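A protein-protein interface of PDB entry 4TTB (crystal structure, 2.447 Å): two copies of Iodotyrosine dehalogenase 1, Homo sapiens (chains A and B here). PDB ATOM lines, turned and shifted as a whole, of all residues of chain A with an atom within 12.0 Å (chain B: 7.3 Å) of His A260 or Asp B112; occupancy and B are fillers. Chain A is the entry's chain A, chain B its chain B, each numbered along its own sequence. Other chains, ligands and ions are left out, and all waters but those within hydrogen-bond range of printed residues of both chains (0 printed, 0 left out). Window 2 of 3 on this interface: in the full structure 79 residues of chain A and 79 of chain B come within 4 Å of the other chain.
The backbone NH of Val B109 is in hydrogen-bond range of the backbone carbonyl oxygen of Val A257, 2.8 Å away. N of Val A259 lies within hydrogen-bond range of O of Val B109, 3.1 Å away. The backbone carbonyl oxygen of Val A259 is in hydrogen-bond range of the backbone NH of Lys B111 (3.2 Å). A ring nitrogen (NE2) of His A260 lies within hydrogen-bond range of the side-chain amino group of Lys B111. The backbone carbonyl oxygen (O) of His A260 sits close to the side-chain carboxylate (OD1) of Asp B112, at 3.2 Å.
The backbone NH (N) of Asp B114 lies within hydrogen-bond range of the side-chain carboxylate (OD2) of Asp B112, at 3.1 Å.
Among the printed residues, merely in contact across the chains: Thr A258 with Met B83 (3.5 Å), Thr A258 with Val B109 (3.5 Å), Val A259 with Asp B112 (3.6 Å) and Thr A258 with Lys B111 (3.8 Å).
His A260 touches just these residues of chain B: Lys B111 (3.0 Å) and Asp B112 (3.2 Å). Asp B112 touches just these residues of chain A: Val A259 (3.6 Å) and His A260 (3.2 Å). No residue of chain A comes within 4 Å of Val B110. Lys B111 touches just these residues of chain A: Thr A258, Val A259 and His A260. Asp B114 touches none of the printed residues of chain A. No residue of chain A comes within 4 Å of Val B115. Lys B116 touches none of the printed residues of chain A. Of the printed residues of chain B, Thr A258 touches Met B83, Val B109 and Lys B111. Of the printed residues of chain B, Val A259 touches Val B109, Lys B111 and Asp B112. Of the printed residues of chain A, Val B109 touches Val A257 (2.8 Å), Thr A258 (3.5 Å) and Val A259 (3.1 Å). Of the printed residues of chain B, Val A257 touches Val B109. Lys B118 touches none of the printed residues of chain A. The nearest residue of chain B that does not touch His A260 is Pro B113 (5.4 Å). The nearest residue of chain A that does not touch Asp B112 is Thr A258 (7.3 Å).
Of the 16 printed residues of chain B, 4 touch a printed residue of chain A. Printed residues of chain B that touch a printed residue of chain A: Met B83, Val B109, Lys B111 and Asp B112. Hydrophobic or aromatic side chains of chain B that line the printed part of chain A: Met B83 and Val B109. Along chain A the printed residues that touch a printed residue of chain B span positions 257 to 260. Among the printed residues, 9 pairs touch across the chains.
No position is printed for both chains. Of the 9 pairs that touch across the chains among the printed residues, none has its exchanged pair printed and touching as well.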
ATOM      1  N   MET A 256      -4.001 -11.348  16.408  1.00  0.00           N
ATOM      2  CA  MET A 256      -3.694 -10.484  15.270  1.00  0.00           C
ATOM      3  C   MET A 256      -4.690  -9.358  15.089  1.00  0.00           C
ATOM      4  O   MET A 256      -5.888  -9.587  15.045  1.00  0.00           O
ATOM      5  CB  MET A 256      -3.620 -11.294  13.971  1.00  0.00           C
ATOM      6  CG  MET A 256      -3.061 -10.496  12.777  1.00  0.00           C
ATOM      7  SD  MET A 256      -3.262 -11.293  11.168  1.00  0.00           S
ATOM      8  CE  MET A 256      -5.041 -11.174  10.939  1.00  0.00           C
ATOM      9  N   VAL A 257      -4.184  -8.141  14.970  1.00  0.00           N
ATOM     10  CA  VAL A 257      -5.026  -6.992  14.686  1.00  0.00           C
ATOM     11  C   VAL A 257      -4.559  -6.365  13.393  1.00  0.00           C
ATOM     12  O   VAL A 257      -3.370  -6.155  13.208  1.00  0.00           O
ATOM     13  CB  VAL A 257      -4.898  -5.935  15.782  1.00  0.00           C
ATOM     14  CG1 VAL A 257      -5.762  -4.729  15.454  1.00  0.00           C
ATOM     15  CG2 VAL A 257      -5.259  -6.530  17.134  1.00  0.00           C
ATOM     16  N   THR A 258      -5.485  -6.069  12.492  1.00  0.00           N
ATOM     17  CA  THR A 258      -5.130  -5.408  11.246  1.00  0.00           C
ATOM     18  C   THR A 258      -5.802  -4.047  11.133  1.00  0.00           C
ATOM     19  O   THR A 258      -7.025  -3.938  11.282  1.00  0.00           O
ATOM     20  CB  THR A 258      -5.530  -6.245  10.024  1.00  0.00           C
ATOM     21  OG1 THR A 258      -4.909  -7.532  10.100  1.00  0.00           O
ATOM     22  CG2 THR A 258      -5.100  -5.538   8.728  1.00  0.00           C
ATOM     23  N   VAL A 259      -5.001  -3.015  10.881  1.00  0.00           N
ATOM     24  CA  VAL A 259      -5.530  -1.687  10.581  1.00  0.00           C
ATOM     25  C   VAL A 259      -5.422  -1.449   9.080  1.00  0.00           C
ATOM     26  O   VAL A 259      -4.327  -1.229   8.560  1.00  0.00           O
ATOM     27  CB  VAL A 259      -4.720  -0.593  11.300  1.00  0.00           C
ATOM     28  CG1 VAL A 259      -5.430   0.751  11.193  1.00  0.00           C
ATOM     29  CG2 VAL A 259      -4.483  -0.977  12.757  1.00  0.00           C
ATOM     30  N   HIS A 260      -6.559  -1.453   8.388  1.00  0.00           N
ATOM     31  CA  HIS A 260      -6.551  -1.407   6.925  1.00  0.00           C
ATOM     32  C   HIS A 260      -7.000  -0.049   6.376  1.00  0.00           C
ATOM     33  O   HIS A 260      -6.469   0.431   5.374  1.00  0.00           O
ATOM     34  CB  HIS A 260      -7.414  -2.543   6.347  1.00  0.00           C
ATOM     35  CG  HIS A 260      -7.045  -2.937   4.946  1.00  0.00           C
ATOM     36  ND1 HIS A 260      -6.277  -2.141   4.122  1.00  0.00           N
ATOM     37  CD2 HIS A 260      -7.338  -4.049   4.227  1.00  0.00           C
ATOM     38  CE1 HIS A 260      -6.116  -2.744   2.955  1.00  0.00           C
ATOM     39  NE2 HIS A 260      -6.750  -3.902   2.994  1.00  0.00           N
ATOM     40  N   GLN B  80       2.561  -4.797  -2.630  1.00  0.00           N
ATOM     41  CA  GLN B  80       1.729  -5.498  -1.656  1.00  0.00           C
ATOM     42  C   GLN B  80       2.119  -6.961  -1.493  1.00  0.00           C
ATOM     43  O   GLN B  80       2.461  -7.642  -2.466  1.00  0.00           O
ATOM     44  CB  GLN B  80       0.243  -5.396  -2.014  1.00  0.00           C
ATOM     45  CG  GLN B  80      -0.377  -4.043  -1.692  1.00  0.00           C
ATOM     46  CD  GLN B  80      -0.148  -3.621  -0.244  1.00  0.00           C
ATOM     47  OE1 GLN B  80      -0.043  -4.462   0.661  1.00  0.00           O
ATOM     48  NE2 GLN B  80      -0.071  -2.307  -0.019  1.00  0.00           N
ATOM     49  N   MET B  83      -2.179 -11.109   1.744  1.00  0.00           N
ATOM     50  CA  MET B  83      -2.572 -11.049   3.141  1.00  0.00           C
ATOM     51  C   MET B  83      -2.579 -12.442   3.757  1.00  0.00           C
ATOM     52  O   MET B  83      -2.301 -12.614   4.942  1.00  0.00           O
ATOM     53  CB  MET B  83      -3.948 -10.410   3.258  1.00  0.00           C
ATOM     54  CG  MET B  83      -4.364 -10.150   4.685  1.00  0.00           C
ATOM     55  SD  MET B  83      -3.098  -9.260   5.611  1.00  0.00           S
ATOM     56  CE  MET B  83      -3.867  -9.266   7.238  1.00  0.00           C
ATOM     57  N   VAL B 109      -0.729  -5.388  12.619  1.00  0.00           N
ATOM     58  CA  VAL B 109      -0.314  -5.275  11.239  1.00  0.00           C
ATOM     59  C   VAL B 109      -0.874  -4.000  10.638  1.00  0.00           C
ATOM     60  O   VAL B 109      -2.082  -3.863  10.457  1.00  0.00           O
ATOM     61  CB  VAL B 109      -0.808  -6.471  10.439  1.00  0.00           C
ATOM     62  CG1 VAL B 109      -0.544  -6.269   8.957  1.00  0.00           C
ATOM     63  CG2 VAL B 109      -0.151  -7.724  10.952  1.00  0.00           C
ATOM     64  N   VAL B 110       0.012  -3.065  10.333  1.00  0.00           N
ATOM     65  CA  VAL B 110      -0.412  -1.776   9.829  1.00  0.00           C
ATOM     66  C   VAL B 110      -0.214  -1.713   8.312  1.00  0.00           C
ATOM     67  O   VAL B 110       0.910  -1.764   7.825  1.00  0.00           O
ATOM     68  CB  VAL B 110       0.374  -0.669  10.541  1.00  0.00           C
ATOM     69  CG1 VAL B 110      -0.212   0.671  10.222  1.00  0.00           C
ATOM     70  CG2 VAL B 110       0.355  -0.937  12.060  1.00  0.00           C
ATOM     71  N   LYS B 111      -1.324  -1.729   7.574  1.00  0.00           N
ATOM     72  CA  LYS B 111      -1.312  -1.541   6.126  1.00  0.00           C
ATOM     73  C   LYS B 111      -1.691  -0.137   5.665  1.00  0.00           C
ATOM     74  O   LYS B 111      -1.626   0.161   4.471  1.00  0.00           O
ATOM     75  CB  LYS B 111      -2.248  -2.550   5.461  1.00  0.00           C
ATOM     76  CG  LYS B 111      -2.067  -3.982   5.935  1.00  0.00           C
ATOM     77  CD  LYS B 111      -3.207  -4.864   5.467  1.00  0.00           C
ATOM     78  CE  LYS B 111      -3.301  -4.921   3.953  1.00  0.00           C
ATOM     79  NZ  LYS B 111      -4.482  -5.718   3.512  1.00  0.00           N
ATOM     80  N   ASP B 112      -2.083   0.731   6.589  1.00  0.00           N
ATOM     81  CA  ASP B 112      -2.633   2.018   6.161  1.00  0.00           C
ATOM     82  C   ASP B 112      -1.558   3.083   6.054  1.00  0.00           C
ATOM     83  O   ASP B 112      -0.925   3.429   7.050  1.00  0.00           O
ATOM     84  CB  ASP B 112      -3.777   2.485   7.062  1.00  0.00           C
ATOM     85  CG  ASP B 112      -4.567   3.631   6.453  1.00  0.00           C
ATOM     86  OD1 ASP B 112      -5.776   3.445   6.183  1.00  0.00           O
ATOM     87  OD2 ASP B 112      -3.987   4.719   6.245  1.00  0.00           O
ATOM     88  N   PRO B 113      -1.362   3.608   4.836  1.00  0.00           N
ATOM     89  CA  PRO B 113      -0.301   4.559   4.487  1.00  0.00           C
ATOM     90  C   PRO B 113      -0.208   5.758   5.427  1.00  0.00           C
ATOM     91  O   PRO B 113       0.905   6.174   5.754  1.00  0.00           O
ATOM     92  CB  PRO B 113      -0.696   5.008   3.080  1.00  0.00           C
ATOM     93  CG  PRO B 113      -1.359   3.817   2.500  1.00  0.00           C
ATOM     94  CD  PRO B 113      -2.161   3.236   3.653  1.00  0.00           C
ATOM     95  N   ASP B 114      -1.346   6.298   5.850  1.00  0.00           N
ATOM     96  CA  ASP B 114      -1.357   7.457   6.737  1.00  0.00           C
ATOM     97  C   ASP B 114      -0.745   7.128   8.090  1.00  0.00           C
ATOM     98  O   ASP B 114       0.179   7.797   8.551  1.00  0.00           O
ATOM     99  CB  ASP B 114      -2.783   7.965   6.952  1.00  0.00           C
ATOM    100  CG  ASP B 114      -3.520   8.200   5.656  1.00  0.00           C
ATOM    101  OD1 ASP B 114      -3.194   9.190   4.963  1.00  0.00           O
ATOM    102  OD2 ASP B 114      -4.433   7.403   5.341  1.00  0.00           O
ATOM    103  N   VAL B 115      -1.268   6.092   8.726  1.00  0.00           N
ATOM    104  CA  VAL B 115      -0.826   5.742  10.066  1.00  0.00           C
ATOM    105  C   VAL B 115       0.598   5.173  10.048  1.00  0.00           C
ATOM    106  O   VAL B 115       1.351   5.354  11.001  1.00  0.00           O
ATOM    107  CB  VAL B 115      -1.859   4.817  10.785  1.00  0.00           C
ATOM    108  CG1 VAL B 115      -2.134   3.584   9.964  1.00  0.00           C
ATOM    109  CG2 VAL B 115      -1.416   4.463  12.206  1.00  0.00           C
ATOM    110  N   LYS B 116       0.983   4.531   8.947  1.00  0.00           N
ATOM    111  CA  LYS B 116       2.366   4.088   8.786  1.00  0.00           C
ATOM    112  C   LYS B 116       3.320   5.282   8.756  1.00  0.00           C
ATOM    113  O   LYS B 116       4.407   5.234   9.329  1.00  0.00           O
ATOM    114  CB  LYS B 116       2.536   3.270   7.504  1.00  0.00           C
ATOM    115  CG  LYS B 116       1.849   1.922   7.505  1.00  0.00           C
ATOM    116  CD  LYS B 116       1.976   1.272   6.141  1.00  0.00           C
ATOM    117  CE  LYS B 116       3.405   1.299   5.674  1.00  0.00           C
ATOM    118  NZ  LYS B 116       3.486   1.182   4.195  1.00  0.00           N
ATOM    119  N   HIS B 117       2.908   6.343   8.064  1.00  0.00           N
ATOM    120  CA  HIS B 117       3.663   7.590   8.032  1.00  0.00           C
ATOM    121  C   HIS B 117       3.716   8.227   9.418  1.00  0.00           C
ATOM    122  O   HIS B 117       4.775   8.654   9.871  1.00  0.00           O
ATOM    123  CB  HIS B 117       3.031   8.562   7.032  1.00  0.00           C
ATOM    124  CG  HIS B 117       3.898   9.738   6.698  1.00  0.00           C
ATOM    125  ND1 HIS B 117       3.992  10.848   7.510  1.00  0.00           N
ATOM    126  CD2 HIS B 117       4.704   9.979   5.636  1.00  0.00           C
ATOM    127  CE1 HIS B 117       4.821  11.722   6.964  1.00  0.00           C
ATOM    128  NE2 HIS B 117       5.265  11.221   5.827  1.00  0.00           N
ATOM    129  N   LYS B 118       2.564   8.290  10.082  1.00  0.00           N
ATOM    130  CA  LYS B 118       2.494   8.776  11.458  1.00  0.00           C
ATOM    131  C   LYS B 118       3.455   7.994  12.338  1.00  0.00           C
ATOM    132  O   LYS B 118       4.160   8.565  13.172  1.00  0.00           O
ATOM    133  CB  LYS B 118       1.069   8.652  11.999  1.00  0.00           C
ATOM    134  CG  LYS B 118       0.081   9.612  11.355  1.00  0.00           C
ATOM    135  CD  LYS B 118      -1.213   9.702  12.145  1.00  0.00           C
ATOM    136  CE  LYS B 118      -2.107  10.816  11.616  1.00  0.00           C
ATOM    137  NZ  LYS B 118      -3.331  10.994  12.454  1.00  0.00           N
ATOM    138  N   ILE B 119       3.472   6.680  12.130  1.00  0.00           N
ATOM    139  CA  ILE B 119       4.418   5.788  12.788  1.00  0.00           C
ATOM    140  C   ILE B 119       5.869   6.160  12.456  1.00  0.00           C
ATOM    141  O   ILE B 119       6.727   6.187  13.343  1.00  0.00           O
ATOM    142  CB  ILE B 119       4.147   4.321  12.390  1.00  0.00           C
ATOM    143  CG1 ILE B 119       2.961   3.768  13.175  1.00  0.00           C
ATOM    144  CG2 ILE B 119       5.348   3.452  12.653  1.00  0.00           C
ATOM    145  CD1 ILE B 119       2.525   2.402  12.712  1.00  0.00           C
ATOM    146  N   PRO B 159       5.101  -2.274   2.318  1.00  0.00           N
ATOM    147  CA  PRO B 159       3.645  -2.322   2.211  1.00  0.00           C
ATOM    148  C   PRO B 159       3.001  -2.538   3.573  1.00  0.00           C
ATOM    149  O   PRO B 159       1.914  -2.008   3.811  1.00  0.00           O
ATOM    150  CB  PRO B 159       3.406  -3.538   1.313  1.00  0.00           C
ATOM    151  CG  PRO B 159       4.588  -4.409   1.559  1.00  0.00           C
ATOM    152  CD  PRO B 159       5.733  -3.452   1.701  1.00  0.00           C
ATOM    153  N   ILE B 160       3.684  -3.276   4.450  1.00  0.00           N
ATOM    154  CA  ILE B 160       3.144  -3.693   5.746  1.00  0.00           C
ATOM    155  C   ILE B 160       4.135  -3.422   6.888  1.00  0.00           C
ATOM    156  O   ILE B 160       5.335  -3.639   6.742  1.00  0.00           O
ATOM    157  CB  ILE B 160       2.776  -5.220   5.722  1.00  0.00           C
ATOM    158  CG1 ILE B 160       1.319  -5.433   5.305  1.00  0.00           C
ATOM    159  CG2 ILE B 160       3.012  -5.880   7.060  1.00  0.00           C
ATOM    160  CD1 ILE B 160       1.023  -5.269   3.812  1.00  0.00           C
ATOM    161  N   LEU B 161       3.632  -2.927   8.016  1.00  0.00           N
ATOM    162  CA  LEU B 161       4.413  -2.892   9.253  1.00  0.00           C
ATOM    163  C   LEU B 161       3.840  -3.875  10.290  1.00  0.00           C
ATOM    164  O   LEU B 161       2.637  -3.878  10.563  1.00  0.00           O
ATOM    165  CB  LEU B 161       4.420  -1.487   9.848  1.00  0.00           C
ATOM    166  CG  LEU B 161       5.099  -0.362   9.051  1.00  0.00           C
ATOM    167  CD1 LEU B 161       4.924   0.971   9.755  1.00  0.00           C
ATOM    168  CD2 LEU B 161       6.567  -0.661   8.852  1.00  0.00           C
